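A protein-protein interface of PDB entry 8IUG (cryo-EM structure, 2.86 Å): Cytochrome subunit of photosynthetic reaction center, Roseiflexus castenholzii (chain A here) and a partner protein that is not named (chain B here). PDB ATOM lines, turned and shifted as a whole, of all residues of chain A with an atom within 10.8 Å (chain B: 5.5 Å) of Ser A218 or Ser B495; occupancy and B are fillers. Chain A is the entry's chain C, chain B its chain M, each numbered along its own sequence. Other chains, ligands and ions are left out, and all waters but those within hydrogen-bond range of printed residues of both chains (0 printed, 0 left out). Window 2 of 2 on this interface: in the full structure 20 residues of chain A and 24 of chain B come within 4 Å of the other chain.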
ATOM      1  N   LEU A 209      -5.930  15.027 -19.113  1.00  0.00           N
ATOM      2  CA  LEU A 209      -5.188  14.714 -17.898  1.00  0.00           C
ATOM      3  C   LEU A 209      -5.688  13.424 -17.268  1.00  0.00           C
ATOM      4  O   LEU A 209      -5.778  13.308 -16.045  1.00  0.00           O
ATOM      5  CB  LEU A 209      -5.278  15.863 -16.895  1.00  0.00           C
ATOM      6  CG  LEU A 209      -4.650  17.211 -17.259  1.00  0.00           C
ATOM      7  CD1 LEU A 209      -5.186  18.296 -16.359  1.00  0.00           C
ATOM      8  CD2 LEU A 209      -3.145  17.153 -17.161  1.00  0.00           C
ATOM      9  N   VAL A 210      -6.018  12.430 -18.087  1.00  0.00           N
ATOM     10  CA  VAL A 210      -6.493  11.138 -17.603  1.00  0.00           C
ATOM     11  C   VAL A 210      -5.327  10.159 -17.615  1.00  0.00           C
ATOM     12  O   VAL A 210      -4.575  10.086 -18.594  1.00  0.00           O
ATOM     13  CB  VAL A 210      -7.677  10.622 -18.441  1.00  0.00           C
ATOM     14  CG1 VAL A 210      -8.865  11.551 -18.298  1.00  0.00           C
ATOM     15  CG2 VAL A 210      -7.303  10.488 -19.893  1.00  0.00           C
ATOM     16  N   VAL A 211      -5.150   9.435 -16.511  1.00  0.00           N
ATOM     17  CA  VAL A 211      -3.989   8.563 -16.347  1.00  0.00           C
ATOM     18  C   VAL A 211      -4.343   7.161 -15.881  1.00  0.00           C
ATOM     19  O   VAL A 211      -3.492   6.260 -15.973  1.00  0.00           O
ATOM     20  CB  VAL A 211      -2.963   9.199 -15.376  1.00  0.00           C
ATOM     21  CG1 VAL A 211      -2.464  10.532 -15.896  1.00  0.00           C
ATOM     22  CG2 VAL A 211      -3.557   9.353 -13.987  1.00  0.00           C
ATOM     23  N   THR A 212      -5.551   6.901 -15.388  1.00  0.00           N
ATOM     24  CA  THR A 212      -5.839   5.637 -14.719  1.00  0.00           C
ATOM     25  C   THR A 212      -5.971   4.502 -15.728  1.00  0.00           C
ATOM     26  O   THR A 212      -6.784   4.576 -16.655  1.00  0.00           O
ATOM     27  CB  THR A 212      -7.112   5.756 -13.887  1.00  0.00           C
ATOM     28  OG1 THR A 212      -6.887   6.643 -12.789  1.00  0.00           O
ATOM     29  CG2 THR A 212      -7.517   4.407 -13.346  1.00  0.00           C
ATOM     30  N   GLY A 213      -5.176   3.450 -15.540  1.00  0.00           N
ATOM     31  CA  GLY A 213      -5.266   2.260 -16.357  1.00  0.00           C
ATOM     32  C   GLY A 213      -4.577   2.330 -17.699  1.00  0.00           C
ATOM     33  O   GLY A 213      -4.713   1.394 -18.492  1.00  0.00           O
ATOM     34  N   ARG A 214      -3.835   3.396 -17.980  1.00  0.00           N
ATOM     35  CA  ARG A 214      -3.229   3.591 -19.288  1.00  0.00           C
ATOM     36  C   ARG A 214      -1.817   3.025 -19.305  1.00  0.00           C
ATOM     37  O   ARG A 214      -0.981   3.397 -18.478  1.00  0.00           O
ATOM     38  CB  ARG A 214      -3.209   5.073 -19.654  1.00  0.00           C
ATOM     39  CG  ARG A 214      -4.580   5.657 -19.885  1.00  0.00           C
ATOM     40  CD  ARG A 214      -4.596   6.499 -21.133  1.00  0.00           C
ATOM     41  NE  ARG A 214      -3.982   7.799 -20.922  1.00  0.00           N
ATOM     42  CZ  ARG A 214      -3.539   8.584 -21.894  1.00  0.00           C
ATOM     43  NH1 ARG A 214      -3.571   8.202 -23.158  1.00  0.00           N
ATOM     44  NH2 ARG A 214      -3.050   9.780 -21.587  1.00  0.00           N
ATOM     45  N   LYS A 215      -1.557   2.131 -20.252  1.00  0.00           N
ATOM     46  CA  LYS A 215      -0.256   1.502 -20.403  1.00  0.00           C
ATOM     47  C   LYS A 215       0.643   2.231 -21.389  1.00  0.00           C
ATOM     48  O   LYS A 215       1.779   1.801 -21.606  1.00  0.00           O
ATOM     49  CB  LYS A 215      -0.426   0.043 -20.827  1.00  0.00           C
ATOM     50  CG  LYS A 215      -1.048  -0.830 -19.756  1.00  0.00           C
ATOM     51  CD  LYS A 215      -1.077  -2.284 -20.170  1.00  0.00           C
ATOM     52  CE  LYS A 215      -1.686  -3.149 -19.085  1.00  0.00           C
ATOM     53  NZ  LYS A 215      -1.861  -4.562 -19.524  1.00  0.00           N
ATOM     54  N   ASP A 216       0.163   3.319 -21.990  1.00  0.00           N
ATOM     55  CA  ASP A 216       0.983   4.220 -22.788  1.00  0.00           C
ATOM     56  C   ASP A 216       1.371   5.472 -22.013  1.00  0.00           C
ATOM     57  O   ASP A 216       1.591   6.527 -22.613  1.00  0.00           O
ATOM     58  CB  ASP A 216       0.249   4.600 -24.071  1.00  0.00           C
ATOM     59  CG  ASP A 216      -1.194   4.980 -23.826  1.00  0.00           C
ATOM     60  OD1 ASP A 216      -1.905   4.209 -23.153  1.00  0.00           O
ATOM     61  OD2 ASP A 216      -1.618   6.051 -24.302  1.00  0.00           O
ATOM     62  N   VAL A 217       1.459   5.366 -20.691  1.00  0.00           N
ATOM     63  CA  VAL A 217       1.650   6.495 -19.792  1.00  0.00           C
ATOM     64  C   VAL A 217       2.432   5.977 -18.593  1.00  0.00           C
ATOM     65  O   VAL A 217       2.363   4.792 -18.257  1.00  0.00           O
ATOM     66  CB  VAL A 217       0.279   7.112 -19.399  1.00  0.00           C
ATOM     67  CG1 VAL A 217       0.262   7.651 -17.982  1.00  0.00           C
ATOM     68  CG2 VAL A 217      -0.099   8.201 -20.374  1.00  0.00           C
ATOM     69  N   SER A 218       3.215   6.852 -17.972  1.00  0.00           N
ATOM     70  CA  SER A 218       4.016   6.467 -16.814  1.00  0.00           C
ATOM     71  C   SER A 218       4.037   7.631 -15.831  1.00  0.00           C
ATOM     72  O   SER A 218       3.211   8.545 -15.902  1.00  0.00           O
ATOM     73  CB  SER A 218       5.416   6.021 -17.246  1.00  0.00           C
ATOM     74  OG  SER A 218       6.039   5.298 -16.206  1.00  0.00           O
ATOM     75  N   ASN A 219       4.981   7.586 -14.885  1.00  0.00           N
ATOM     76  CA  ASN A 219       5.014   8.517 -13.759  1.00  0.00           C
ATOM     77  C   ASN A 219       5.273   9.963 -14.170  1.00  0.00           C
ATOM     78  O   ASN A 219       4.922  10.874 -13.414  1.00  0.00           O
ATOM     79  CB  ASN A 219       6.071   8.064 -12.752  1.00  0.00           C
ATOM     80  CG  ASN A 219       5.600   6.907 -11.883  1.00  0.00           C
ATOM     81  OD1 ASN A 219       4.546   6.328 -12.116  1.00  0.00           O
ATOM     82  ND2 ASN A 219       6.386   6.574 -10.874  1.00  0.00           N
ATOM     83  N   HIS A 220       5.874  10.198 -15.336  1.00  0.00           N
ATOM     84  CA  HIS A 220       6.038  11.560 -15.834  1.00  0.00           C
ATOM     85  C   HIS A 220       4.682  12.221 -16.075  1.00  0.00           C
ATOM     86  O   HIS A 220       4.436  13.361 -15.652  1.00  0.00           O
ATOM     87  CB  HIS A 220       6.873  11.521 -17.116  1.00  0.00           C
ATOM     88  CG  HIS A 220       7.421  12.849 -17.540  1.00  0.00           C
ATOM     89  ND1 HIS A 220       7.057  13.462 -18.719  1.00  0.00           N
ATOM     90  CD2 HIS A 220       8.324  13.669 -16.953  1.00  0.00           C
ATOM     91  CE1 HIS A 220       7.699  14.609 -18.833  1.00  0.00           C
ATOM     92  NE2 HIS A 220       8.476  14.759 -17.775  1.00  0.00           N
ATOM     93  N   GLU A 221       3.769  11.492 -16.719  1.00  0.00           N
ATOM     94  CA  GLU A 221       2.433  12.013 -16.969  1.00  0.00           C
ATOM     95  C   GLU A 221       1.635  12.150 -15.680  1.00  0.00           C
ATOM     96  O   GLU A 221       0.840  13.084 -15.536  1.00  0.00           O
ATOM     97  CB  GLU A 221       1.703  11.115 -17.962  1.00  0.00           C
ATOM     98  CG  GLU A 221       2.199  11.232 -19.389  1.00  0.00           C
ATOM     99  CD  GLU A 221       3.499  10.493 -19.633  1.00  0.00           C
ATOM    100  OE1 GLU A 221       3.843   9.603 -18.834  1.00  0.00           O
ATOM    101  OE2 GLU A 221       4.181  10.801 -20.629  1.00  0.00           O
ATOM    102  N   VAL A 222       1.830  11.240 -14.728  1.00  0.00           N
ATOM    103  CA  VAL A 222       1.124  11.350 -13.455  1.00  0.00           C
ATOM    104  C   VAL A 222       1.590  12.583 -12.690  1.00  0.00           C
ATOM    105  O   VAL A 222       0.789  13.267 -12.044  1.00  0.00           O
ATOM    106  CB  VAL A 222       1.294  10.065 -12.626  1.00  0.00           C
ATOM    107  CG1 VAL A 222       0.331  10.073 -11.459  1.00  0.00           C
ATOM    108  CG2 VAL A 222       1.063   8.839 -13.485  1.00  0.00           C
ATOM    109  N   GLU A 223       2.886  12.897 -12.759  1.00  0.00           N
ATOM    110  CA  GLU A 223       3.384  14.120 -12.133  1.00  0.00           C
ATOM    111  C   GLU A 223       2.805  15.364 -12.798  1.00  0.00           C
ATOM    112  O   GLU A 223       2.442  16.337 -12.119  1.00  0.00           O
ATOM    113  CB  GLU A 223       4.906  14.146 -12.196  1.00  0.00           C
ATOM    114  CG  GLU A 223       5.535  15.257 -11.400  1.00  0.00           C
ATOM    115  CD  GLU A 223       7.034  15.305 -11.561  1.00  0.00           C
ATOM    116  OE1 GLU A 223       7.510  15.229 -12.710  1.00  0.00           O
ATOM    117  OE2 GLU A 223       7.737  15.408 -10.537  1.00  0.00           O
ATOM    118  N   GLN A 224       2.723  15.355 -14.131  1.00  0.00           N
ATOM    119  CA  GLN A 224       2.129  16.489 -14.831  1.00  0.00           C
ATOM    120  C   GLN A 224       0.651  16.651 -14.493  1.00  0.00           C
ATOM    121  O   GLN A 224       0.138  17.773 -14.482  1.00  0.00           O
ATOM    122  CB  GLN A 224       2.319  16.333 -16.336  1.00  0.00           C
ATOM    123  CG  GLN A 224       3.768  16.372 -16.773  1.00  0.00           C
ATOM    124  CD  GLN A 224       4.449  17.676 -16.419  1.00  0.00           C
ATOM    125  OE1 GLN A 224       5.511  17.685 -15.800  1.00  0.00           O
ATOM    126  NE2 GLN A 224       3.845  18.785 -16.818  1.00  0.00           N
ATOM    127  N   ASN A 225      -0.047  15.542 -14.244  1.00  0.00           N
ATOM    128  CA  ASN A 225      -1.426  15.596 -13.764  1.00  0.00           C
ATOM    129  C   ASN A 225      -1.502  16.212 -12.369  1.00  0.00           C
ATOM    130  O   ASN A 225      -2.343  17.080 -12.101  1.00  0.00           O
ATOM    131  CB  ASN A 225      -2.010  14.178 -13.780  1.00  0.00           C
ATOM    132  CG  ASN A 225      -3.345  14.068 -13.069  1.00  0.00           C
ATOM    133  OD1 ASN A 225      -4.391  14.344 -13.642  1.00  0.00           O
ATOM    134  ND2 ASN A 225      -3.313  13.625 -11.823  1.00  0.00           N
ATOM    135  N   GLN A 226      -0.609  15.784 -11.474  1.00  0.00           N
ATOM    136  CA  GLN A 226      -0.677  16.205 -10.079  1.00  0.00           C
ATOM    137  C   GLN A 226      -0.373  17.687  -9.905  1.00  0.00           C
ATOM    138  O   GLN A 226      -0.946  18.330  -9.017  1.00  0.00           O
ATOM    139  CB  GLN A 226       0.275  15.367  -9.234  1.00  0.00           C
ATOM    140  CG  GLN A 226      -0.208  13.956  -8.993  1.00  0.00           C
ATOM    141  CD  GLN A 226      -1.517  13.918  -8.245  1.00  0.00           C
ATOM    142  OE1 GLN A 226      -2.577  13.727  -8.834  1.00  0.00           O
ATOM    143  NE2 GLN A 226      -1.451  14.101  -6.938  1.00  0.00           N
ATOM    144  N   PRO B 419      14.517   8.792 -13.377  1.00  0.00           N
ATOM    145  CA  PRO B 419      14.803   7.895 -14.494  1.00  0.00           C
ATOM    146  C   PRO B 419      14.388   8.522 -15.811  1.00  0.00           C
ATOM    147  O   PRO B 419      13.588   9.467 -15.829  1.00  0.00           O
ATOM    148  CB  PRO B 419      13.962   6.652 -14.172  1.00  0.00           C
ATOM    149  CG  PRO B 419      12.981   7.084 -13.180  1.00  0.00           C
ATOM    150  CD  PRO B 419      13.587   8.186 -12.412  1.00  0.00           C
ATOM    151  N   PRO B 420      14.918   8.040 -16.933  1.00  0.00           N
ATOM    152  CA  PRO B 420      14.589   8.637 -18.229  1.00  0.00           C
ATOM    153  C   PRO B 420      13.094   8.613 -18.487  1.00  0.00           C
ATOM    154  O   PRO B 420      12.411   7.639 -18.143  1.00  0.00           O
ATOM    155  CB  PRO B 420      15.346   7.752 -19.232  1.00  0.00           C
ATOM    156  CG  PRO B 420      15.839   6.589 -18.468  1.00  0.00           C
ATOM    157  CD  PRO B 420      15.966   7.017 -17.055  1.00  0.00           C
ATOM    158  N   PRO B 421      12.546   9.674 -19.097  1.00  0.00           N
ATOM    159  CA  PRO B 421      11.088   9.767 -19.268  1.00  0.00           C
ATOM    160  C   PRO B 421      10.511   8.716 -20.204  1.00  0.00           C
ATOM    161  O   PRO B 421      11.235   7.871 -20.733  1.00  0.00           O
ATOM    162  CB  PRO B 421      10.894  11.183 -19.822  1.00  0.00           C
ATOM    163  CG  PRO B 421      12.207  11.566 -20.378  1.00  0.00           C
ATOM    164  CD  PRO B 421      13.227  10.906 -19.524  1.00  0.00           C
ATOM    165  N   THR B 422       9.192   8.760 -20.404  1.00  0.00           N
ATOM    166  CA  THR B 422       8.496   7.684 -21.100  1.00  0.00           C
ATOM    167  C   THR B 422       8.797   7.651 -22.594  1.00  0.00           C
ATOM    168  O   THR B 422       8.610   6.604 -23.222  1.00  0.00           O
ATOM    169  CB  THR B 422       6.987   7.810 -20.874  1.00  0.00           C
ATOM    170  OG1 THR B 422       6.739   8.197 -19.518  1.00  0.00           O
ATOM    171  CG2 THR B 422       6.290   6.493 -21.134  1.00  0.00           C
ATOM    172  N   ASN B 493       9.397   0.634 -19.477  1.00  0.00           N
ATOM    173  CA  ASN B 493      10.028   1.943 -19.393  1.00  0.00           C
ATOM    174  C   ASN B 493      10.740   2.084 -18.056  1.00  0.00           C
ATOM    175  O   ASN B 493      10.381   1.434 -17.074  1.00  0.00           O
ATOM    176  CB  ASN B 493       9.009   3.076 -19.588  1.00  0.00           C
ATOM    177  CG  ASN B 493       7.726   2.858 -18.814  1.00  0.00           C
ATOM    178  OD1 ASN B 493       7.737   2.365 -17.693  1.00  0.00           O
ATOM    179  ND2 ASN B 493       6.609   3.225 -19.418  1.00  0.00           N
ATOM    180  N   TRP B 494      11.763   2.939 -18.032  1.00  0.00           N
ATOM    181  CA  TRP B 494      12.524   3.180 -16.812  1.00  0.00           C
ATOM    182  C   TRP B 494      11.840   4.148 -15.864  1.00  0.00           C
ATOM    183  O   TRP B 494      12.161   4.148 -14.675  1.00  0.00           O
ATOM    184  CB  TRP B 494      13.918   3.720 -17.135  1.00  0.00           C
ATOM    185  CG  TRP B 494      14.899   2.702 -17.601  1.00  0.00           C
ATOM    186  CD1 TRP B 494      15.581   2.708 -18.774  1.00  0.00           C
ATOM    187  CD2 TRP B 494      15.319   1.529 -16.899  1.00  0.00           C
ATOM    188  NE1 TRP B 494      16.402   1.614 -18.852  1.00  0.00           N
ATOM    189  CE2 TRP B 494      16.258   0.873 -17.712  1.00  0.00           C
ATOM    190  CE3 TRP B 494      14.991   0.968 -15.661  1.00  0.00           C
ATOM    191  CZ2 TRP B 494      16.870  -0.314 -17.331  1.00  0.00           C
ATOM    192  CZ3 TRP B 494      15.598  -0.207 -15.286  1.00  0.00           C
ATOM    193  CH2 TRP B 494      16.528  -0.837 -16.117  1.00  0.00           C
ATOM    194  N   SER B 495      10.914   4.968 -16.351  1.00  0.00           N
ATOM    195  CA  SER B 495      10.247   5.940 -15.488  1.00  0.00           C
ATOM    196  C   SER B 495       9.205   5.325 -14.603  1.00  0.00           C
ATOM    197  O   SER B 495       8.459   6.069 -13.969  1.00  0.00           O
ATOM    198  CB  SER B 495       9.616   7.048 -16.325  1.00  0.00           C
ATOM    199  OG  SER B 495       8.522   6.556 -17.064  1.00  0.00           O
ATOM    200  N   ALA B 496       9.117   4.002 -14.534  1.00  0.00           N
ATOM    201  CA  ALA B 496       8.221   3.319 -13.617  1.00  0.00           C
ATOM    202  C   ALA B 496       8.847   3.092 -12.250  1.00  0.00           C
ATOM    203  O   ALA B 496       8.175   2.570 -11.356  1.00  0.00           O
ATOM    204  CB  ALA B 496       7.789   1.978 -14.214  1.00  0.00           C
ATOM    205  N   ALA B 497      10.123   3.475 -12.068  1.00  0.00           N
ATOM    206  CA  ALA B 497      11.039   3.339 -10.950  1.00  0.00           C
ATOM    207  C   ALA B 497      11.182   4.660 -10.201  1.00  0.00           C
ATOM    208  O   ALA B 497      10.986   5.731 -10.776  1.00  0.00           O
ATOM    209  CB  ALA B 497      12.410   2.878 -11.444  1.00  0.00           C
ATOM    210  N   HIS B 515      -1.924   5.639 -10.460  1.00  0.00           N
ATOM    211  CA  HIS B 515      -1.903   5.163 -11.840  1.00  0.00           C
ATOM    212  C   HIS B 515      -2.736   3.899 -12.012  1.00  0.00           C
ATOM    213  O   HIS B 515      -3.530   3.791 -12.951  1.00  0.00           O
ATOM    214  CB  HIS B 515      -0.454   4.917 -12.257  1.00  0.00           C
ATOM    215  CG  HIS B 515      -0.262   4.686 -13.723  1.00  0.00           C
ATOM    216  ND1 HIS B 515       0.977   4.449 -14.275  1.00  0.00           N
ATOM    217  CD2 HIS B 515      -1.142   4.658 -14.751  1.00  0.00           C
ATOM    218  CE1 HIS B 515       0.852   4.282 -15.577  1.00  0.00           C
ATOM    219  NE2 HIS B 515      -0.423   4.405 -15.893  1.00  0.00           N
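Among the printed residues, pairs that only touch across the chains: Val A211 with His B515 (3.1 Å), Thr A212 with His B515 (3.4 Å), Val A217 with His B515 (3.1 Å), Ser A218 with Thr B422 (3.4 Å), Ser A218 with Asn B493 (3.7 Å), Ser A218 with Ala B496 (3.7 Å) and Asn A219 with Ser B495 (3.3 Å).
NH1 of Arg A214 is in salt-bridge range of OD2 of Asp A216 (3.1 Å). The backbone NH of Ser A218 is in hydrogen-bond range of the side-chain carboxylate of Glu A221 (3.0 Å). O of Val A210 is in hydrogen-bond range of NE of Arg A214, 3.3 Å away. The side-chain hydroxyl of Thr B422 is in hydrogen-bond range of the side-chain hydroxyl of Ser B495 (3.4 Å).
Of the 10 printed residues of chain B, 5 touch a printed residue of chain A. Printed residues of chain B that touch a printed residue of chain A: Thr B422, Asn B493, Ser B495, Ala B496 and His B515. Of the 18 printed residues of chain A, 8 touch a printed residue of chain B. Printed residues of chain A that touch a printed residue of chain B: Val A211, Thr A212, Gly A213, Arg A214, Val A217, Ser A218, Asn A219 and Glu A221. Among the printed residues, 11 pairs touch across the chains. Among the printed residues, no Asp or Glu carboxylate lies within 4 Å of a Lys or Arg side-chain nitrogen of the other chain.
Printed residues of chain B within 4 Å of Gly A213: His B515. Printed residues of chain B within 4 Å of Arg A214: His B515 (2.8 Å). Ser A218 touches four residues of chain B. Printed residues of chain B within 4 Å of Asn A219: Ser B495 (3.3 Å). Gln A224 touches none of the printed residues of chain B. No residue of chain A comes within 4 Å of Pro B419. No residue of chain A comes within 4 Å of Pro B421. Thr B422 touches just these residues of chain A: Ser A218 and Glu A221. Of chain A, only Ser A218 comes within 4 Å of Asn B493. Ser B495 touches two residues of chain A. Printed residues of chain A within 4 Å of His B515: Val A211, Thr A212, Gly A213, Arg A214 and Val A217. The nearest residue of chain B that does not touch Ser A218 is His B515 (4.04 Å).
The backbone carbonyl oxygen (O) of Arg A214 sits at hydrogen-bond distance from a ring nitrogen (NE2) of His B515 (2.8 Å). The side-chain hydroxyl (OG) of Ser A218 sits at hydrogen-bond distance from the side-chain hydroxyl (OG) of Ser B495, 2.9 Å away. The backbone NH (N) of Gly A213 sits at hydrogen-bond distance from the backbone carbonyl oxygen (O) of His B515 (3.1 Å). The side-chain carboxylate (OE1) of Glu A221 lies within hydrogen-bond range of the side-chain hydroxyl (OG1) of Thr B422, at 3.3 Å.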
